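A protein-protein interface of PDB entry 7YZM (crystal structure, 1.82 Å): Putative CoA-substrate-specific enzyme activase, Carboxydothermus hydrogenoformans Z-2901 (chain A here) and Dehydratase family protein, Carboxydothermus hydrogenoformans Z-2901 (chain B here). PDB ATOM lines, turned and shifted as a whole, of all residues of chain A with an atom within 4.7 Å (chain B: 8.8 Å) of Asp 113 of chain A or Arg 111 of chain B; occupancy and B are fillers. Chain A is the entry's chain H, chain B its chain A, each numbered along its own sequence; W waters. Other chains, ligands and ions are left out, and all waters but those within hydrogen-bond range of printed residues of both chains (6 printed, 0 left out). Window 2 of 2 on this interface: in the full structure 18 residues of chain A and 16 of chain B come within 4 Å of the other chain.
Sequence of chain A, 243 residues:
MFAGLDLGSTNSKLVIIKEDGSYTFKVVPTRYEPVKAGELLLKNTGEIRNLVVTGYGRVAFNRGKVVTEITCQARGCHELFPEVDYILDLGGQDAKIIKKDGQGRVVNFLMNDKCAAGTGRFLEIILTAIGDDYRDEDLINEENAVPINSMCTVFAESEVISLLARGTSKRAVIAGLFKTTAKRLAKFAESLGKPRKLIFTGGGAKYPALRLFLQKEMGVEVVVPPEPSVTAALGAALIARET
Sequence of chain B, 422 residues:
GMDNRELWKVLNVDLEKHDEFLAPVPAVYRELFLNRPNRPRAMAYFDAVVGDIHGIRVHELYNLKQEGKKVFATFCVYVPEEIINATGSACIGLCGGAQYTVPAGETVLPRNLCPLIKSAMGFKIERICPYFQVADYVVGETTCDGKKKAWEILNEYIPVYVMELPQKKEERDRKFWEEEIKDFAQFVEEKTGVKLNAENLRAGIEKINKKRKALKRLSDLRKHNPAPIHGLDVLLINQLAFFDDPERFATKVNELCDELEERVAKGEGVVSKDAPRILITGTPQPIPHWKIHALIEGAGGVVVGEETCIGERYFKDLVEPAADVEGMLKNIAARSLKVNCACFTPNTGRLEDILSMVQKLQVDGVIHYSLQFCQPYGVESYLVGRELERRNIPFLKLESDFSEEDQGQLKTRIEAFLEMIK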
ATOM      1  N   MET A 111     -30.074 -15.132 -26.707  1.00  0.00           N
ATOM      2  CA  MET A 111     -29.748 -14.371 -25.508  1.00  0.00           C
ATOM      3  C   MET A 111     -28.333 -13.814 -25.633  1.00  0.00           C
ATOM      4  O   MET A 111     -27.561 -14.198 -26.513  1.00  0.00           O
ATOM      5  CB  MET A 111     -29.900 -15.231 -24.244  1.00  0.00           C
ATOM      6  CG  MET A 111     -31.336 -15.736 -24.030  1.00  0.00           C
ATOM      7  SD  MET A 111     -31.597 -16.726 -22.541  1.00  0.00           S
ATOM      8  CE  MET A 111     -31.128 -15.571 -21.251  1.00  0.00           C
ATOM      9  N   ASN A 112     -28.000 -12.876 -24.749  1.00  0.00           N
ATOM     10  CA  ASN A 112     -26.709 -12.206 -24.824  1.00  0.00           C
ATOM     11  C   ASN A 112     -25.563 -13.214 -24.741  1.00  0.00           C
ATOM     12  O   ASN A 112     -25.698 -14.295 -24.159  1.00  0.00           O
ATOM     13  CB  ASN A 112     -26.585 -11.192 -23.690  1.00  0.00           C
ATOM     14  CG  ASN A 112     -26.771 -11.827 -22.320  1.00  0.00           C
ATOM     15  OD1 ASN A 112     -27.896 -12.036 -21.872  1.00  0.00           O
ATOM     16  ND2 ASN A 112     -25.662 -12.142 -21.654  1.00  0.00           N
ATOM     17  N   ASP A 113     -24.423 -12.855 -25.335  1.00  0.00           N
ATOM     18  CA  ASP A 113     -23.210 -13.633 -25.135  1.00  0.00           C
ATOM     19  C   ASP A 113     -22.623 -13.328 -23.754  1.00  0.00           C
ATOM     20  O   ASP A 113     -23.082 -12.434 -23.043  1.00  0.00           O
ATOM     21  CB  ASP A 113     -22.191 -13.373 -26.256  1.00  0.00           C
ATOM     22  CG  ASP A 113     -21.693 -11.929 -26.317  1.00  0.00           C
ATOM     23  OD1 ASP A 113     -21.348 -11.342 -25.270  1.00  0.00           O
ATOM     24  OD2 ASP A 113     -21.594 -11.392 -27.445  1.00  0.00           O
ATOM     25  N   LYS A 114     -21.597 -14.096 -23.376  1.00  0.00           N
ATOM     26  CA  LYS A 114     -21.050 -13.987 -22.023  1.00  0.00           C
ATOM     27  C   LYS A 114     -20.536 -12.581 -21.739  1.00  0.00           C
ATOM     28  O   LYS A 114     -20.740 -12.043 -20.642  1.00  0.00           O
ATOM     29  CB  LYS A 114     -19.927 -15.012 -21.817  1.00  0.00           C
ATOM     30  CG  LYS A 114     -20.400 -16.415 -21.415  1.00  0.00           C
ATOM     31  CD  LYS A 114     -19.225 -17.386 -21.193  1.00  0.00           C
ATOM     32  CE  LYS A 114     -18.632 -17.305 -19.776  1.00  0.00           C
ATOM     33  NZ  LYS A 114     -19.572 -16.805 -18.718  1.00  0.00           N
ATOM     34  N   CYS A 115     -19.850 -11.970 -22.710  1.00  0.00           N
ATOM     35  CA  CYS A 115     -19.279 -10.651 -22.484  1.00  0.00           C
ATOM     36  C   CYS A 115     -20.340  -9.569 -22.387  1.00  0.00           C
ATOM     37  O   CYS A 115     -20.036  -8.457 -21.942  1.00  0.00           O
ATOM     38  CB  CYS A 115     -18.297 -10.297 -23.595  1.00  0.00           C
ATOM     39  SG  CYS A 115     -16.812 -11.316 -23.620  1.00  0.00           S
ATOM     40  N   ALA A 116     -21.571  -9.862 -22.798  1.00  0.00           N
ATOM     41  CA  ALA A 116     -22.653  -8.893 -22.776  1.00  0.00           C
ATOM     42  C   ALA A 116     -23.541  -9.047 -21.549  1.00  0.00           C
ATOM     43  O   ALA A 116     -24.595  -8.405 -21.476  1.00  0.00           O
ATOM     44  CB  ALA A 116     -23.492  -9.016 -24.050  1.00  0.00           C
ATOM     45  N   ALA A 117     -23.136  -9.878 -20.591  1.00  0.00           N
ATOM     46  CA  ALA A 117     -23.925 -10.100 -19.390  1.00  0.00           C
ATOM     47  C   ALA A 117     -23.906  -8.872 -18.485  1.00  0.00           C
ATOM     48  O   ALA A 117     -22.929  -8.117 -18.435  1.00  0.00           O
ATOM     49  CB  ALA A 117     -23.394 -11.312 -18.620  1.00  0.00           C
ATOM     50  N   SER A 150     -18.851  -0.357 -26.239  1.00  0.00           N
ATOM     51  CA  SER A 150     -19.984  -1.272 -26.284  1.00  0.00           C
ATOM     52  C   SER A 150     -19.597  -2.716 -25.978  1.00  0.00           C
ATOM     53  O   SER A 150     -20.440  -3.612 -26.084  1.00  0.00           O
ATOM     54  CB  SER A 150     -20.656  -1.211 -27.662  1.00  0.00           C
ATOM     55  OG  SER A 150     -19.706  -1.350 -28.706  1.00  0.00           O
ATOM     56  N   MET A 151     -18.348  -2.968 -25.595  1.00  0.00           N
ATOM     57  CA  MET A 151     -17.909  -4.347 -25.415  1.00  0.00           C
ATOM     58  C   MET A 151     -18.603  -5.010 -24.233  1.00  0.00           C
ATOM     59  O   MET A 151     -19.208  -6.079 -24.366  1.00  0.00           O
ATOM     60  CB  MET A 151     -16.400  -4.394 -25.220  1.00  0.00           C
ATOM     61  CG  MET A 151     -15.862  -5.796 -25.097  1.00  0.00           C
ATOM     62  SD  MET A 151     -15.503  -6.329 -26.789  1.00  0.00           S
ATOM     63  CE  MET A 151     -16.142  -7.966 -26.796  1.00  0.00           C
ATOM     64  N   ARG A 184     -26.398  -0.934 -29.235  1.00  0.00           N
ATOM     65  CA  ARG A 184     -26.138  -2.370 -29.154  1.00  0.00           C
ATOM     66  C   ARG A 184     -27.439  -3.165 -29.171  1.00  0.00           C
ATOM     67  O   ARG A 184     -27.526  -4.230 -29.796  1.00  0.00           O
ATOM     68  CB  ARG A 184     -25.372  -2.724 -27.882  1.00  0.00           C
ATOM     69  CG  ARG A 184     -24.014  -2.110 -27.702  1.00  0.00           C
ATOM     70  CD  ARG A 184     -23.563  -2.383 -26.256  1.00  0.00           C
ATOM     71  NE  ARG A 184     -23.325  -3.807 -25.987  1.00  0.00           N
ATOM     72  CZ  ARG A 184     -23.035  -4.306 -24.786  1.00  0.00           C
ATOM     73  NH1 ARG A 184     -22.817  -5.608 -24.631  1.00  0.00           N
ATOM     74  NH2 ARG A 184     -22.963  -3.505 -23.732  1.00  0.00           N
ATOM     75  N   GLN B  99     -14.366   3.170 -34.198  1.00  0.00           N
ATOM     76  CA  GLN B  99     -15.319   2.509 -33.316  1.00  0.00           C
ATOM     77  C   GLN B  99     -16.747   2.618 -33.839  1.00  0.00           C
ATOM     78  O   GLN B  99     -17.585   1.765 -33.521  1.00  0.00           O
ATOM     79  CB  GLN B  99     -15.239   3.110 -31.914  1.00  0.00           C
ATOM     80  CG  GLN B  99     -16.194   2.474 -30.907  1.00  0.00           C
ATOM     81  CD  GLN B  99     -15.815   1.049 -30.541  1.00  0.00           C
ATOM     82  OE1 GLN B  99     -14.651   0.661 -30.629  1.00  0.00           O
ATOM     83  NE2 GLN B  99     -16.803   0.260 -30.129  1.00  0.00           N
ATOM     84  N   VAL B 102     -18.137  -0.546 -35.410  1.00  0.00           N
ATOM     85  CA  VAL B 102     -17.917  -1.848 -34.791  1.00  0.00           C
ATOM     86  C   VAL B 102     -19.232  -2.554 -34.486  1.00  0.00           C
ATOM     87  O   VAL B 102     -19.348  -3.751 -34.790  1.00  0.00           O
ATOM     88  CB  VAL B 102     -17.015  -1.702 -33.553  1.00  0.00           C
ATOM     89  CG1 VAL B 102     -17.120  -2.940 -32.679  1.00  0.00           C
ATOM     90  CG2 VAL B 102     -15.567  -1.477 -33.987  1.00  0.00           C
ATOM     91  N   PRO B 103     -20.245  -1.905 -33.901  1.00  0.00           N
ATOM     92  CA  PRO B 103     -21.498  -2.639 -33.640  1.00  0.00           C
ATOM     93  C   PRO B 103     -22.139  -3.205 -34.898  1.00  0.00           C
ATOM     94  O   PRO B 103     -22.719  -4.298 -34.845  1.00  0.00           O
ATOM     95  CB  PRO B 103     -22.388  -1.588 -32.961  1.00  0.00           C
ATOM     96  CG  PRO B 103     -21.426  -0.634 -32.346  1.00  0.00           C
ATOM     97  CD  PRO B 103     -20.265  -0.558 -33.304  1.00  0.00           C
ATOM     98  N   GLY B 105     -20.435  -4.227 -37.603  1.00  0.00           N
ATOM     99  CA  GLY B 105     -19.638  -5.388 -37.934  1.00  0.00           C
ATOM    100  C   GLY B 105     -20.007  -6.579 -37.081  1.00  0.00           C
ATOM    101  O   GLY B 105     -19.970  -7.721 -37.549  1.00  0.00           O
ATOM    102  N   GLU B 106     -20.399  -6.330 -35.833  1.00  0.00           N
ATOM    103  CA  GLU B 106     -20.776  -7.394 -34.914  1.00  0.00           C
ATOM    104  C   GLU B 106     -22.119  -8.032 -35.250  1.00  0.00           C
ATOM    105  O   GLU B 106     -22.497  -9.009 -34.589  1.00  0.00           O
ATOM    106  CB  GLU B 106     -20.814  -6.853 -33.481  1.00  0.00           C
ATOM    107  CG  GLU B 106     -19.446  -6.476 -32.923  1.00  0.00           C
ATOM    108  CD  GLU B 106     -19.506  -5.734 -31.597  1.00  0.00           C
ATOM    109  OE1 GLU B 106     -20.614  -5.318 -31.181  1.00  0.00           O
ATOM    110  OE2 GLU B 106     -18.429  -5.569 -30.971  1.00  0.00           O
ATOM    111  N   THR B 107     -22.856  -7.528 -36.246  1.00  0.00           N
ATOM    112  CA  THR B 107     -24.062  -8.240 -36.654  1.00  0.00           C
ATOM    113  C   THR B 107     -23.727  -9.552 -37.357  1.00  0.00           C
ATOM    114  O   THR B 107     -24.580 -10.443 -37.418  1.00  0.00           O
ATOM    115  CB  THR B 107     -24.951  -7.384 -37.568  1.00  0.00           C
ATOM    116  OG1 THR B 107     -24.238  -7.017 -38.755  1.00  0.00           O
ATOM    117  CG2 THR B 107     -25.426  -6.123 -36.851  1.00  0.00           C
ATOM    118  N   VAL B 108     -22.502  -9.697 -37.874  1.00  0.00           N
ATOM    119  CA  VAL B 108     -22.115 -10.897 -38.606  1.00  0.00           C
ATOM    120  C   VAL B 108     -20.800 -11.476 -38.094  1.00  0.00           C
ATOM    121  O   VAL B 108     -20.373 -12.546 -38.541  1.00  0.00           O
ATOM    122  CB  VAL B 108     -22.008 -10.619 -40.121  1.00  0.00           C
ATOM    123  CG1 VAL B 108     -23.295 -10.010 -40.663  1.00  0.00           C
ATOM    124  CG2 VAL B 108     -20.820  -9.707 -40.425  1.00  0.00           C
ATOM    125  N   LEU B 109     -20.145 -10.779 -37.170  1.00  0.00           N
ATOM    126  CA  LEU B 109     -18.873 -11.224 -36.627  1.00  0.00           C
ATOM    127  C   LEU B 109     -18.946 -11.331 -35.110  1.00  0.00           C
ATOM    128  O   LEU B 109     -19.737 -10.627 -34.476  1.00  0.00           O
ATOM    129  CB  LEU B 109     -17.745 -10.257 -36.997  1.00  0.00           C
ATOM    130  CG  LEU B 109     -17.339 -10.151 -38.465  1.00  0.00           C
ATOM    131  CD1 LEU B 109     -16.394  -8.957 -38.643  1.00  0.00           C
ATOM    132  CD2 LEU B 109     -16.708 -11.438 -38.943  1.00  0.00           C
ATOM    133  N   PRO B 110     -18.117 -12.189 -34.496  1.00  0.00           N
ATOM    134  CA  PRO B 110     -18.078 -12.255 -33.027  1.00  0.00           C
ATOM    135  C   PRO B 110     -17.610 -10.942 -32.425  1.00  0.00           C
ATOM    136  O   PRO B 110     -16.770 -10.243 -32.987  1.00  0.00           O
ATOM    137  CB  PRO B 110     -17.071 -13.382 -32.741  1.00  0.00           C
ATOM    138  CG  PRO B 110     -16.904 -14.123 -34.028  1.00  0.00           C
ATOM    139  CD  PRO B 110     -17.165 -13.125 -35.120  1.00  0.00           C
ATOM    140  N   ARG B 111     -18.145 -10.621 -31.245  1.00  0.00           N
ATOM    141  CA  ARG B 111     -17.735  -9.388 -30.579  1.00  0.00           C
ATOM    142  C   ARG B 111     -16.316  -9.493 -30.020  1.00  0.00           C
ATOM    143  O   ARG B 111     -15.624  -8.471 -29.914  1.00  0.00           O
ATOM    144  CB  ARG B 111     -18.767  -9.028 -29.502  1.00  0.00           C
ATOM    145  CG  ARG B 111     -20.191  -8.770 -30.090  1.00  0.00           C
ATOM    146  CD  ARG B 111     -21.199  -8.165 -29.092  1.00  0.00           C
ATOM    147  NE  ARG B 111     -20.983  -8.693 -27.750  1.00  0.00           N
ATOM    148  CZ  ARG B 111     -20.612  -7.953 -26.710  1.00  0.00           C
ATOM    149  NH1 ARG B 111     -20.404  -8.526 -25.535  1.00  0.00           N
ATOM    150  NH2 ARG B 111     -20.450  -6.644 -26.842  1.00  0.00           N
ATOM    151  N   ASN B 112     -15.846 -10.702 -29.699  1.00  0.00           N
ATOM    152  CA  ASN B 112     -14.462 -10.912 -29.256  1.00  0.00           C
ATOM    153  C   ASN B 112     -13.535 -11.148 -30.449  1.00  0.00           C
ATOM    154  O   ASN B 112     -12.862 -12.173 -30.559  1.00  0.00           O
ATOM    155  CB  ASN B 112     -14.363 -12.098 -28.303  1.00  0.00           C
ATOM    156  CG  ASN B 112     -15.044 -11.864 -26.990  1.00  0.00           C
ATOM    157  OD1 ASN B 112     -15.090 -10.747 -26.486  1.00  0.00           O
ATOM    158  ND2 ASN B 112     -15.572 -12.935 -26.411  1.00  0.00           N
ATOM    159  N   LEU B 113     -13.527 -10.188 -31.364  1.00  0.00           N
ATOM    160  CA  LEU B 113     -12.688 -10.238 -32.550  1.00  0.00           C
ATOM    161  C   LEU B 113     -11.960  -8.912 -32.651  1.00  0.00           C
ATOM    162  O   LEU B 113     -12.366  -7.915 -32.047  1.00  0.00           O
ATOM    163  CB  LEU B 113     -13.503 -10.499 -33.817  1.00  0.00           C
ATOM    164  CG  LEU B 113     -12.791 -11.139 -35.009  1.00  0.00           C
ATOM    165  CD1 LEU B 113     -12.588 -12.625 -34.778  1.00  0.00           C
ATOM    166  CD2 LEU B 113     -13.574 -10.905 -36.295  1.00  0.00           C
ATOM    167  N   CYS B 114     -10.878  -8.918 -33.408  1.00  0.00           N
ATOM    168  CA  CYS B 114     -10.081  -7.721 -33.598  1.00  0.00           C
ATOM    169  C   CYS B 114     -10.951  -6.564 -34.082  1.00  0.00           C
ATOM    170  O   CYS B 114     -11.714  -6.730 -35.047  1.00  0.00           O
ATOM    171  CB  CYS B 114      -8.989  -7.977 -34.625  1.00  0.00           C
ATOM    172  SG  CYS B 114      -8.008  -6.531 -34.980  1.00  0.00           S
ATOM    173  N   PRO B 115     -10.818  -5.373 -33.496  1.00  0.00           N
ATOM    174  CA  PRO B 115     -11.636  -4.243 -33.963  1.00  0.00           C
ATOM    175  C   PRO B 115     -11.312  -3.802 -35.378  1.00  0.00           C
ATOM    176  O   PRO B 115     -12.179  -3.217 -36.034  1.00  0.00           O
ATOM    177  CB  PRO B 115     -11.330  -3.137 -32.944  1.00  0.00           C
ATOM    178  CG  PRO B 115     -10.038  -3.519 -32.313  1.00  0.00           C
ATOM    179  CD  PRO B 115      -9.962  -5.014 -32.348  1.00  0.00           C
ATOM    180  N   LYS B 118     -13.729  -5.897 -37.357  1.00  0.00           N
ATOM    181  CA  LYS B 118     -15.118  -5.561 -37.082  1.00  0.00           C
ATOM    182  C   LYS B 118     -15.478  -4.214 -37.692  1.00  0.00           C
ATOM    183  O   LYS B 118     -16.567  -4.045 -38.252  1.00  0.00           O
ATOM    184  CB  LYS B 118     -15.356  -5.542 -35.571  1.00  0.00           C
ATOM    185  CG  LYS B 118     -15.201  -6.889 -34.893  1.00  0.00           C
ATOM    186  CD  LYS B 118     -15.737  -6.861 -33.470  1.00  0.00           C
ATOM    187  CE  LYS B 118     -14.849  -6.054 -32.544  1.00  0.00           C
ATOM    188  NZ  LYS B 118     -15.391  -6.029 -31.156  1.00  0.00           N
ATOM    189  N   GLN B 372      -6.837  -5.297 -29.123  1.00  0.00           N
ATOM    190  CA  GLN B 372      -7.548  -6.330 -28.380  1.00  0.00           C
ATOM    191  C   GLN B 372      -8.004  -7.454 -29.307  1.00  0.00           C
ATOM    192  O   GLN B 372      -8.515  -7.208 -30.405  1.00  0.00           O
ATOM    193  CB  GLN B 372      -8.740  -5.701 -27.654  1.00  0.00           C
ATOM    194  CG  GLN B 372      -9.398  -6.603 -26.629  1.00  0.00           C
ATOM    195  CD  GLN B 372      -8.877  -6.389 -25.219  1.00  0.00           C
ATOM    196  OE1 GLN B 372      -7.953  -5.606 -24.990  1.00  0.00           O
ATOM    197  NE2 GLN B 372      -9.471  -7.094 -24.266  1.00  0.00           N
ATOM    198  N   PHE B 373      -7.784  -8.695 -28.859  1.00  0.00           N
ATOM    199  CA  PHE B 373      -8.151  -9.939 -29.532  1.00  0.00           C
ATOM    200  C   PHE B 373      -7.324 -10.210 -30.783  1.00  0.00           C
ATOM    201  O   PHE B 373      -7.660 -11.112 -31.559  1.00  0.00           O
ATOM    202  CB  PHE B 373      -9.651  -9.974 -29.866  1.00  0.00           C
ATOM    203  CG  PHE B 373     -10.529  -9.599 -28.700  1.00  0.00           C
ATOM    204  CD1 PHE B 373     -10.554 -10.382 -27.554  1.00  0.00           C
ATOM    205  CD2 PHE B 373     -11.306  -8.456 -28.736  1.00  0.00           C
ATOM    206  CE1 PHE B 373     -11.344 -10.030 -26.468  1.00  0.00           C
ATOM    207  CE2 PHE B 373     -12.098  -8.103 -27.658  1.00  0.00           C
ATOM    208  CZ  PHE B 373     -12.110  -8.890 -26.519  1.00  0.00           C
ATOM    209  N   ASP B 401      -8.710  -1.037 -27.830  1.00  0.00           N
ATOM    210  CA  ASP B 401      -9.557  -1.118 -29.014  1.00  0.00           C
ATOM    211  C   ASP B 401      -9.755   0.293 -29.557  1.00  0.00           C
ATOM    212  O   ASP B 401      -9.015   1.215 -29.195  1.00  0.00           O
ATOM    213  CB  ASP B 401     -10.889  -1.807 -28.697  1.00  0.00           C
ATOM    214  CG  ASP B 401     -11.656  -1.140 -27.568  1.00  0.00           C
ATOM    215  OD1 ASP B 401     -11.578   0.099 -27.433  1.00  0.00           O
ATOM    216  OD2 ASP B 401     -12.353  -1.864 -26.819  1.00  0.00           O
HETATM  217  O   HOH W   1     -12.693  -4.726 -27.532  1.00  0.00           O
HETATM  218  O   HOH W   2     -18.025  -3.999 -28.886  1.00  0.00           O
HETATM  219  O   HOH W   3     -20.227 -12.343 -29.867  1.00  0.00           O
HETATM  220  O   HOH W   4     -18.535 -13.036 -25.566  1.00  0.00           O
HETATM  221  O   HOH W   5     -19.652   1.040 -29.954  1.00  0.00           O
HETATM  222  O   HOH W   6     -20.897  -4.601 -28.685  1.00  0.00           O
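The side-chain carboxylate of Asp 113 of chain A lies within salt-bridge range of the guanidinium group of Arg 111 of chain B, at 2.8 Å.
NH2 of Arg 111 of chain B sits at hydrogen-bond distance from O of Ser 150 of chain A (3.1 Å).
O of Met 151 of chain A is in hydrogen-bond range of NH2 of Arg 111 of chain B, at 2.8 Å.
The side-chain amide oxygen (OD1) of Asn 112 of chain B sits close to the side-chain sulfur (SG) of Cys 115 of chain A, at 3.4 Å.
The guanidinium group of Arg 111 of chain B sits close to the backbone NH of Ala 116 of chain A, at 3.3 Å.
The guanidinium group of Arg 184 of chain A sits close to the guanidinium group of Arg 111 of chain B, 3.4 Å away.
The backbone carbonyl oxygen (O) of Arg 111 of chain B lies within hydrogen-bond range of the side-chain amino group (NZ) of Lys 118 of chain B (2.7 Å).
OD1 of Asp 113 of chain A is in hydrogen-bond range of N of Cys 115 of chain A (3.0 Å).
The backbone NH (N) of Ala 116 of chain A sits at hydrogen-bond distance from the side-chain carboxylate (OD1) of Asp 113 of chain A (2.9 Å).
The backbone carbonyl oxygen (O) of Ser 150 of chain A lies within hydrogen-bond range of the guanidinium group (NE) of Arg 184 of chain A (2.9 Å).
C of Cys 115 of chain A touches NH1 of Arg 111 of chain B, at 3.3 Å.
NE2 of Gln 99 of chain B touches OG of Ser 150 of chain A, at 3.6 Å.
Met 151 of chain A touches Asn 112 of chain B.
Met 151 of chain A touches Phe 373 of chain B (SD to CE2, 3.9 Å).
Of chain B, only Arg 111 comes within 4 Å of Asp 113 of chain A.
Arg 111 of chain B touches just these residues of chain A: Asp 113, Cys 115, Ala 116, Ser 150, Met 151 and Arg 184.
Of the printed residues of chain B, Met 151 of chain A touches Arg 111 (2.8 Å), Asn 112 (3.0 Å) and Phe 373 (3.9 Å).
Printed residues of chain B within 4 Å of Arg 184 of chain A: Arg 111.
Printed residues of chain B within 4 Å of Cys 115 of chain A: Arg 111 (3.3 Å) and Asn 112 (3.4 Å).
Printed residues of chain B within 4 Å of Ser 150 of chain A: Gln 99 (3.6 Å) and Arg 111 (3.1 Å).
Of the printed residues of chain A, Phe 373 of chain B touches Met 151 (3.9 Å).
Pro 115 of chain B touches none of the printed residues of chain A.
Asp 401 of chain B touches none of the printed residues of chain A.
The nearest residue of chain B that does not touch Asp 113 of chain A is Asn 112 of chain B (6.1 Å).
The nearest printed residue of chain A that does not touch Gln 99 of chain B is Met 151 of chain A (5.8 Å).
Hydrophobic or aromatic side chains of chain A that line the printed part of chain B: Ala 116 and Met 151.
Of the 18 printed residues of chain B, 4 touch a printed residue of chain A.
Printed residues of chain B that touch a printed residue of chain A: Gln 99, Arg 111, Asn 112 and Phe 373.
Hydrophobic or aromatic side chains of chain B that line the printed part of chain A: Phe 373.
Among the printed residues, Asp or Glu carboxylates within 4 Å of a Lys or Arg side-chain nitrogen of the other chain: Asp 113 of chain A with Arg 111 of chain B.
Water W6 lies within hydrogen-bond range of OE1 of Glu 106 of chain B (2.6 Å), NH2 of Arg 111 of chain B (2.8 Å) and O of Ser 150 of chain A (2.8 Å).
Water W2 lies within hydrogen-bond range of OE2 of Glu 106 of chain B (2.6 Å), OG of Ser 150 of chain A (3.1 Å) and N of Met 151 of chain A (3.5 Å).
Water W5 lies within hydrogen-bond range of the side-chain hydroxyl (OG) of Ser 150 of chain A (2.7 Å) and the side-chain amide nitrogen (NE2) of Gln 99 of chain B (3.0 Å).
Water W3 bridges OD2 of Asp 113 of chain A (2.9 Å) and N of Arg 111 of chain B (3.0 Å).
Water W1 bridges OD2 of Asp 401 of chain B (3.0 Å) and SD of Met 151 of chain A (3.3 Å).
Water W4 lies within hydrogen-bond range of the side-chain amide nitrogen of Asn 112 of chain B (3.1 Å), the side-chain carboxylate of Asp 113 of chain A (3.3 Å) and the backbone NH of Cys 115 of chain A (3.3 Å).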
